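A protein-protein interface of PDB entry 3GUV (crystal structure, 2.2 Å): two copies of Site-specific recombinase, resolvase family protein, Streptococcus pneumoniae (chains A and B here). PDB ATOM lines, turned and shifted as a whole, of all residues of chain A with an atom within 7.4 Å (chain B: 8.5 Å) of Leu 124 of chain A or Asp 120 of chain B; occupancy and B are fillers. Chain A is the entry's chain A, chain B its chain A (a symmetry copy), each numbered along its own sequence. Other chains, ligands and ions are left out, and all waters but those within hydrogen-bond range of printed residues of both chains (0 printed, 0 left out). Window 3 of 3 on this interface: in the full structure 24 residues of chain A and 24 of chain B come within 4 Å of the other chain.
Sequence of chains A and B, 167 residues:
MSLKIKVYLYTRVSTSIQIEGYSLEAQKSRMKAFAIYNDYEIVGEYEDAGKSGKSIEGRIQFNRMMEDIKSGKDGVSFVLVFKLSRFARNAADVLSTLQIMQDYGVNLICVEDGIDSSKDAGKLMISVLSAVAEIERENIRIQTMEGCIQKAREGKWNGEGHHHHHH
The side-chain carboxylate of Asp 120 of chain B lies within hydrogen-bond range of the backbone NH of Met 125 of chain B.
The backbone carbonyl oxygen of Lys 123 of chain A lies within hydrogen-bond range of the side-chain hydroxyl of Ser 127 of chain A (3.4 Å).
N of Leu 124 of chain A sits at hydrogen-bond distance from OD2 of Asp 120 of chain A.
OD2 of Asp 120 of chain A sits at hydrogen-bond distance from N of Met 125 of chain A (2.9 Å).
N of Leu 124 of chain B sits at hydrogen-bond distance from OD2 of Asp 120 of chain B (3.0 Å).
Asp 120 of chain A touches Leu 124 of chain B, and with the chains exchanged Leu 124 of chain A touches Asp 120 of chain B.
Positions printed for both chains: 120, 123, 124, 125, 126, 127, 128 and 129.
Of the 4 pairs that touch across the chains among the printed residues, 2 have their exchanged pair printed and touching as well.
Asp 120 of chain A touches Leu 124 of chain B.
Leu 124 of chain A touches Asp 120 of chain B (CD2 to OD1, 3.4 Å).
Ser 127 of chain A touches Ile 115 of chain B.
Val 128 of chain A touches Ile 115 of chain B (CA to CD1, 3.9 Å).
Of the 19 printed residues of chain B, 3 touch a printed residue of chain A.
Hydrophobic or aromatic side chains of chain B that line the printed part of chain A: Ile 115 and Leu 124.
Along chain B the printed residues that touch a printed residue of chain A span positions 115 to 124.
Among the printed residues, no Asp or Glu carboxylate lies within 4 Å of a Lys or Arg side-chain nitrogen of the other chain.
Of chain B, only Asp 120 comes within 4 Å of Leu 124 of chain A.
Asp 120 of chain B touches just one residue of chain A: Leu 124 (3.4 Å).
Printed residues of chain B within 4 Å of Ser 127 of chain A: Ile 115 (3.8 Å).
Of the printed residues of chain A, Ile 115 of chain B touches Ser 127 (3.8 Å) and Val 128 (3.9 Å).
The nearest residue of chain A that does not touch Asp 120 of chain B is Asp 120 of chain A (7.2 Å).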
ATOM      1  N   ASP A 120      -3.287 -18.083  -7.157  1.00  0.00           N
ATOM      2  CA  ASP A 120      -2.989 -18.955  -6.020  1.00  0.00           C
ATOM      3  C   ASP A 120      -3.367 -18.295  -4.677  1.00  0.00           C
ATOM      4  O   ASP A 120      -2.638 -17.451  -4.143  1.00  0.00           O
ATOM      5  CB  ASP A 120      -1.499 -19.350  -6.057  1.00  0.00           C
ATOM      6  CG  ASP A 120      -1.233 -20.719  -5.440  1.00  0.00           C
ATOM      7  OD1 ASP A 120      -2.220 -21.437  -5.130  1.00  0.00           O
ATOM      8  OD2 ASP A 120      -0.034 -21.071  -5.270  1.00  0.00           O
ATOM      9  N   LYS A 123      -0.604 -19.690  -1.449  1.00  0.00           N
ATOM     10  CA  LYS A 123       0.482 -20.256  -2.263  1.00  0.00           C
ATOM     11  C   LYS A 123       0.416 -21.805  -2.355  1.00  0.00           C
ATOM     12  O   LYS A 123       1.422 -22.465  -2.137  1.00  0.00           O
ATOM     13  CB  LYS A 123       1.837 -19.828  -1.679  1.00  0.00           C
ATOM     14  N   LEU A 124      -0.749 -22.371  -2.693  1.00  0.00           N
ATOM     15  CA  LEU A 124      -0.941 -23.851  -2.710  1.00  0.00           C
ATOM     16  C   LEU A 124      -0.141 -24.602  -3.783  1.00  0.00           C
ATOM     17  O   LEU A 124       0.327 -25.733  -3.550  1.00  0.00           O
ATOM     18  CB  LEU A 124      -2.423 -24.200  -2.884  1.00  0.00           C
ATOM     19  CG  LEU A 124      -2.732 -25.707  -2.980  1.00  0.00           C
ATOM     20  CD1 LEU A 124      -2.363 -26.461  -1.676  1.00  0.00           C
ATOM     21  CD2 LEU A 124      -4.177 -25.943  -3.355  1.00  0.00           C
ATOM     22  N   MET A 125      -0.025 -23.989  -4.963  1.00  0.00           N
ATOM     23  CA  MET A 125       0.771 -24.517  -6.071  1.00  0.00           C
ATOM     24  C   MET A 125       2.206 -24.776  -5.649  1.00  0.00           C
ATOM     25  O   MET A 125       2.740 -25.837  -5.931  1.00  0.00           O
ATOM     26  CB  MET A 125       0.750 -23.542  -7.265  1.00  0.00           C
ATOM     27  CG  MET A 125       1.548 -24.001  -8.511  1.00  0.00           C
ATOM     28  SD  MET A 125       0.983 -23.263 -10.080  1.00  0.00           S
ATOM     29  CE  MET A 125       1.932 -24.244 -11.261  1.00  0.00           C
ATOM     30  N   ILE A 126       2.819 -23.805  -4.974  1.00  0.00           N
ATOM     31  CA  ILE A 126       4.205 -23.909  -4.501  1.00  0.00           C
ATOM     32  C   ILE A 126       4.332 -25.064  -3.465  1.00  0.00           C
ATOM     33  O   ILE A 126       5.289 -25.843  -3.527  1.00  0.00           O
ATOM     34  CB  ILE A 126       4.753 -22.543  -3.903  1.00  0.00           C
ATOM     35  CG1 ILE A 126       4.986 -21.492  -5.022  1.00  0.00           C
ATOM     36  CG2 ILE A 126       6.072 -22.749  -3.088  1.00  0.00           C
ATOM     37  CD1 ILE A 126       6.356 -21.664  -5.794  1.00  0.00           C
ATOM     38  N   SER A 127       3.341 -25.200  -2.574  1.00  0.00           N
ATOM     39  CA  SER A 127       3.357 -26.256  -1.523  1.00  0.00           C
ATOM     40  C   SER A 127       3.307 -27.672  -2.093  1.00  0.00           C
ATOM     41  O   SER A 127       4.029 -28.551  -1.634  1.00  0.00           O
ATOM     42  CB  SER A 127       2.177 -26.088  -0.563  1.00  0.00           C
ATOM     43  OG  SER A 127       2.264 -24.865   0.147  1.00  0.00           O
ATOM     44  N   VAL A 128       2.432 -27.881  -3.087  1.00  0.00           N
ATOM     45  CA  VAL A 128       2.277 -29.181  -3.709  1.00  0.00           C
ATOM     46  C   VAL A 128       3.568 -29.509  -4.432  1.00  0.00           C
ATOM     47  O   VAL A 128       4.142 -30.591  -4.265  1.00  0.00           O
ATOM     48  CB  VAL A 128       1.054 -29.208  -4.669  1.00  0.00           C
ATOM     49  CG1 VAL A 128       0.983 -30.515  -5.414  1.00  0.00           C
ATOM     50  CG2 VAL A 128      -0.246 -28.973  -3.878  1.00  0.00           C
ATOM     51  N   LEU A 129       4.042 -28.556  -5.223  1.00  0.00           N
ATOM     52  CA  LEU A 129       5.232 -28.759  -6.059  1.00  0.00           C
ATOM     53  C   LEU A 129       6.462 -29.084  -5.177  1.00  0.00           C
ATOM     54  O   LEU A 129       7.249 -30.014  -5.453  1.00  0.00           O
ATOM     55  CB  LEU A 129       5.509 -27.506  -6.930  1.00  0.00           C
ATOM     56  CG  LEU A 129       4.834 -27.299  -8.305  1.00  0.00           C
ATOM     57  CD1 LEU A 129       5.183 -25.910  -8.845  1.00  0.00           C
ATOM     58  CD2 LEU A 129       5.193 -28.381  -9.325  1.00  0.00           C
ATOM     59  N   SER A 130       6.617 -28.287  -4.125  1.00  0.00           N
ATOM     60  CA  SER A 130       7.641 -28.517  -3.137  1.00  0.00           C
ATOM     61  C   SER A 130       7.507 -29.929  -2.535  1.00  0.00           C
ATOM     62  O   SER A 130       8.500 -30.655  -2.451  1.00  0.00           O
ATOM     63  CB  SER A 130       7.576 -27.445  -2.040  1.00  0.00           C
ATOM     64  OG  SER A 130       8.598 -27.727  -1.119  1.00  0.00           O
ATOM     65  N   LEU B  98      -5.364 -39.867  -4.204  1.00  0.00           N
ATOM     66  CA  LEU B  98      -6.223 -38.745  -3.832  1.00  0.00           C
ATOM     67  C   LEU B  98      -7.579 -38.783  -4.535  1.00  0.00           C
ATOM     68  O   LEU B  98      -8.557 -38.361  -3.971  1.00  0.00           O
ATOM     69  CB  LEU B  98      -5.551 -37.391  -4.133  1.00  0.00           C
ATOM     70  CG  LEU B  98      -6.309 -36.145  -3.636  1.00  0.00           C
ATOM     71  CD1 LEU B  98      -6.755 -36.261  -2.141  1.00  0.00           C
ATOM     72  CD2 LEU B  98      -5.422 -34.956  -3.794  1.00  0.00           C
ATOM     73  N   GLN B 102     -11.176 -39.136  -2.556  1.00  0.00           N
ATOM     74  CA  GLN B 102     -12.236 -38.132  -2.699  1.00  0.00           C
ATOM     75  C   GLN B 102     -13.511 -38.739  -3.330  1.00  0.00           C
ATOM     76  O   GLN B 102     -14.610 -38.325  -2.966  1.00  0.00           O
ATOM     77  CB  GLN B 102     -11.770 -36.913  -3.493  1.00  0.00           C
ATOM     78  CG  GLN B 102     -10.667 -36.109  -2.830  1.00  0.00           C
ATOM     79  CD  GLN B 102     -10.256 -34.878  -3.639  1.00  0.00           C
ATOM     80  OE1 GLN B 102      -9.920 -34.974  -4.820  1.00  0.00           O
ATOM     81  NE2 GLN B 102     -10.272 -33.714  -2.991  1.00  0.00           N
ATOM     82  N   ASN B 107     -10.758 -36.585   2.185  1.00  0.00           N
ATOM     83  CA  ASN B 107      -9.681 -35.658   1.845  1.00  0.00           C
ATOM     84  C   ASN B 107      -8.353 -35.916   2.592  1.00  0.00           C
ATOM     85  O   ASN B 107      -8.287 -36.702   3.550  1.00  0.00           O
ATOM     86  CB  ASN B 107     -10.167 -34.224   2.037  1.00  0.00           C
ATOM     87  CG  ASN B 107     -10.980 -33.724   0.840  1.00  0.00           C
ATOM     88  OD1 ASN B 107     -10.435 -33.428  -0.221  1.00  0.00           O
ATOM     89  ND2 ASN B 107     -12.288 -33.659   1.013  1.00  0.00           N
ATOM     90  N   LEU B 108      -7.296 -35.273   2.118  1.00  0.00           N
ATOM     91  CA  LEU B 108      -5.936 -35.494   2.595  1.00  0.00           C
ATOM     92  C   LEU B 108      -5.377 -34.245   3.255  1.00  0.00           C
ATOM     93  O   LEU B 108      -5.469 -33.140   2.678  1.00  0.00           O
ATOM     94  CB  LEU B 108      -5.021 -35.912   1.453  1.00  0.00           C
ATOM     95  CG  LEU B 108      -3.578 -36.290   1.867  1.00  0.00           C
ATOM     96  CD1 LEU B 108      -3.539 -37.669   2.603  1.00  0.00           C
ATOM     97  CD2 LEU B 108      -2.718 -36.285   0.566  1.00  0.00           C
ATOM     98  N   ASP B 113       3.584 -30.344   5.535  1.00  0.00           N
ATOM     99  CA  ASP B 113       3.475 -29.492   4.330  1.00  0.00           C
ATOM    100  C   ASP B 113       2.392 -28.409   4.455  1.00  0.00           C
ATOM    101  O   ASP B 113       2.380 -27.455   3.683  1.00  0.00           O
ATOM    102  CB  ASP B 113       3.176 -30.340   3.096  1.00  0.00           C
ATOM    103  CG  ASP B 113       4.200 -31.469   2.878  1.00  0.00           C
ATOM    104  OD1 ASP B 113       5.394 -31.250   3.196  1.00  0.00           O
ATOM    105  OD2 ASP B 113       3.822 -32.571   2.377  1.00  0.00           O
ATOM    106  N   GLY B 114       1.486 -28.551   5.419  1.00  0.00           N
ATOM    107  CA  GLY B 114       0.347 -27.646   5.548  1.00  0.00           C
ATOM    108  C   GLY B 114      -0.689 -27.734   4.422  1.00  0.00           C
ATOM    109  O   GLY B 114      -1.419 -26.776   4.184  1.00  0.00           O
ATOM    110  N   ILE B 115      -0.744 -28.869   3.731  1.00  0.00           N
ATOM    111  CA  ILE B 115      -1.615 -29.051   2.578  1.00  0.00           C
ATOM    112  C   ILE B 115      -2.896 -29.722   3.070  1.00  0.00           C
ATOM    113  O   ILE B 115      -2.840 -30.646   3.868  1.00  0.00           O
ATOM    114  CB  ILE B 115      -0.973 -29.978   1.506  1.00  0.00           C
ATOM    115  CG1 ILE B 115       0.182 -29.292   0.751  1.00  0.00           C
ATOM    116  CG2 ILE B 115      -2.025 -30.435   0.523  1.00  0.00           C
ATOM    117  CD1 ILE B 115       0.938 -30.248  -0.227  1.00  0.00           C
ATOM    118  N   ASP B 116      -4.037 -29.223   2.610  1.00  0.00           N
ATOM    119  CA  ASP B 116      -5.346 -29.763   2.963  1.00  0.00           C
ATOM    120  C   ASP B 116      -6.172 -29.731   1.674  1.00  0.00           C
ATOM    121  O   ASP B 116      -6.530 -28.633   1.183  1.00  0.00           O
ATOM    122  CB  ASP B 116      -5.983 -28.905   4.073  1.00  0.00           C
ATOM    123  CG  ASP B 116      -7.438 -29.277   4.375  1.00  0.00           C
ATOM    124  OD1 ASP B 116      -8.079 -30.036   3.598  1.00  0.00           O
ATOM    125  OD2 ASP B 116      -7.947 -28.794   5.418  1.00  0.00           O
ATOM    126  N   SER B 117      -6.428 -30.912   1.104  1.00  0.00           N
ATOM    127  CA  SER B 117      -7.115 -31.011  -0.164  1.00  0.00           C
ATOM    128  C   SER B 117      -8.600 -30.554  -0.147  1.00  0.00           C
ATOM    129  O   SER B 117      -9.143 -30.246  -1.197  1.00  0.00           O
ATOM    130  CB  SER B 117      -6.974 -32.421  -0.746  1.00  0.00           C
ATOM    131  OG  SER B 117      -7.724 -33.392  -0.038  1.00  0.00           O
ATOM    132  N   SER B 118      -9.237 -30.477   1.018  1.00  0.00           N
ATOM    133  CA  SER B 118     -10.633 -30.004   1.120  1.00  0.00           C
ATOM    134  C   SER B 118     -10.751 -28.478   0.922  1.00  0.00           C
ATOM    135  O   SER B 118     -11.796 -27.998   0.516  1.00  0.00           O
ATOM    136  CB  SER B 118     -11.244 -30.377   2.474  1.00  0.00           C
ATOM    137  OG  SER B 118     -10.747 -29.535   3.507  1.00  0.00           O
ATOM    138  N   LYS B 119      -9.678 -27.735   1.216  1.00  0.00           N
ATOM    139  CA  LYS B 119      -9.637 -26.282   1.018  1.00  0.00           C
ATOM    140  C   LYS B 119      -9.339 -25.886  -0.431  1.00  0.00           C
ATOM    141  O   LYS B 119      -9.066 -24.732  -0.691  1.00  0.00           O
ATOM    142  CB  LYS B 119      -8.582 -25.647   1.925  1.00  0.00           C
ATOM    143  CG  LYS B 119      -8.839 -25.852   3.400  1.00  0.00           C
ATOM    144  CD  LYS B 119     -10.124 -25.179   3.839  1.00  0.00           C
ATOM    145  CE  LYS B 119     -10.056 -24.794   5.306  1.00  0.00           C
ATOM    146  NZ  LYS B 119      -9.677 -25.950   6.180  1.00  0.00           N
ATOM    147  N   ASP B 120      -9.410 -26.834  -1.363  1.00  0.00           N
ATOM    148  CA  ASP B 120      -9.070 -26.584  -2.764  1.00  0.00           C
ATOM    149  C   ASP B 120     -10.180 -25.794  -3.490  1.00  0.00           C
ATOM    150  O   ASP B 120     -11.205 -26.348  -3.901  1.00  0.00           O
ATOM    151  CB  ASP B 120      -8.777 -27.925  -3.466  1.00  0.00           C
ATOM    152  CG  ASP B 120      -7.777 -27.791  -4.608  1.00  0.00           C
ATOM    153  OD1 ASP B 120      -7.182 -26.690  -4.755  1.00  0.00           O
ATOM    154  OD2 ASP B 120      -7.587 -28.791  -5.353  1.00  0.00           O
ATOM    155  N   LYS B 123     -10.318 -26.956  -7.806  1.00  0.00           N
ATOM    156  CA  LYS B 123      -9.542 -28.204  -7.764  1.00  0.00           C
ATOM    157  C   LYS B 123      -8.079 -28.017  -8.251  1.00  0.00           C
ATOM    158  O   LYS B 123      -7.615 -28.788  -9.079  1.00  0.00           O
ATOM    159  CB  LYS B 123     -10.240 -29.272  -8.620  1.00  0.00           C
ATOM    160  N   LEU B 124      -7.360 -27.015  -7.728  1.00  0.00           N
ATOM    161  CA  LEU B 124      -5.983 -26.690  -8.203  1.00  0.00           C
ATOM    162  C   LEU B 124      -4.920 -27.755  -7.902  1.00  0.00           C
ATOM    163  O   LEU B 124      -3.998 -27.977  -8.711  1.00  0.00           O
ATOM    164  CB  LEU B 124      -5.510 -25.358  -7.611  1.00  0.00           C
ATOM    165  CG  LEU B 124      -4.070 -24.952  -7.983  1.00  0.00           C
ATOM    166  CD1 LEU B 124      -3.908 -24.715  -9.507  1.00  0.00           C
ATOM    167  CD2 LEU B 124      -3.625 -23.743  -7.193  1.00  0.00           C
ATOM    168  N   MET B 125      -5.028 -28.376  -6.725  1.00  0.00           N
ATOM    169  CA  MET B 125      -4.155 -29.473  -6.309  1.00  0.00           C
ATOM    170  C   MET B 125      -4.164 -30.603  -7.322  1.00  0.00           C
ATOM    171  O   MET B 125      -3.109 -31.090  -7.698  1.00  0.00           O
ATOM    172  CB  MET B 125      -4.583 -30.010  -4.929  1.00  0.00           C
ATOM    173  CG  MET B 125      -3.719 -31.170  -4.371  1.00  0.00           C
ATOM    174  SD  MET B 125      -3.752 -31.326  -2.554  1.00  0.00           S
ATOM    175  CE  MET B 125      -2.443 -32.544  -2.309  1.00  0.00           C
ATOM    176  N   ILE B 126      -5.355 -31.011  -7.757  1.00  0.00           N
ATOM    177  CA  ILE B 126      -5.524 -32.094  -8.735  1.00  0.00           C
ATOM    178  C   ILE B 126      -4.874 -31.694 -10.093  1.00  0.00           C
ATOM    179  O   ILE B 126      -4.188 -32.515 -10.712  1.00  0.00           O
ATOM    180  CB  ILE B 126      -7.043 -32.512  -8.930  1.00  0.00           C
ATOM    181  CG1 ILE B 126      -7.583 -33.264  -7.683  1.00  0.00           C
ATOM    182  CG2 ILE B 126      -7.247 -33.391 -10.207  1.00  0.00           C
ATOM    183  CD1 ILE B 126      -7.203 -34.798  -7.638  1.00  0.00           C
ATOM    184  N   SER B 127      -5.041 -30.430 -10.504  1.00  0.00           N
ATOM    185  CA  SER B 127      -4.483 -29.933 -11.793  1.00  0.00           C
ATOM    186  C   SER B 127      -2.955 -29.955 -11.835  1.00  0.00           C
ATOM    187  O   SER B 127      -2.369 -30.352 -12.836  1.00  0.00           O
ATOM    188  CB  SER B 127      -4.945 -28.502 -12.072  1.00  0.00           C
ATOM    189  OG  SER B 127      -6.351 -28.440 -12.236  1.00  0.00           O
ATOM    190  N   VAL B 128      -2.325 -29.508 -10.740  1.00  0.00           N
ATOM    191  CA  VAL B 128      -0.879 -29.467 -10.653  1.00  0.00           C
ATOM    192  C   VAL B 128      -0.369 -30.894 -10.676  1.00  0.00           C
ATOM    193  O   VAL B 128       0.527 -31.243 -11.453  1.00  0.00           O
ATOM    194  CB  VAL B 128      -0.410 -28.707  -9.380  1.00  0.00           C
ATOM    195  CG1 VAL B 128       1.086 -28.787  -9.227  1.00  0.00           C
ATOM    196  CG2 VAL B 128      -0.861 -27.235  -9.445  1.00  0.00           C
ATOM    197  N   LEU B 129      -0.962 -31.730  -9.836  1.00  0.00           N
ATOM    198  CA  LEU B 129      -0.516 -33.120  -9.678  1.00  0.00           C
ATOM    199  C   LEU B 129      -0.633 -33.880 -11.021  1.00  0.00           C
ATOM    200  O   LEU B 129       0.284 -34.611 -11.452  1.00  0.00           O
ATOM    201  CB  LEU B 129      -1.343 -33.839  -8.579  1.00  0.00           C
ATOM    202  CG  LEU B 129      -0.957 -33.763  -7.085  1.00  0.00           C
ATOM    203  CD1 LEU B 129      -2.042 -34.435  -6.240  1.00  0.00           C
ATOM    204  CD2 LEU B 129       0.415 -34.368  -6.782  1.00  0.00           C
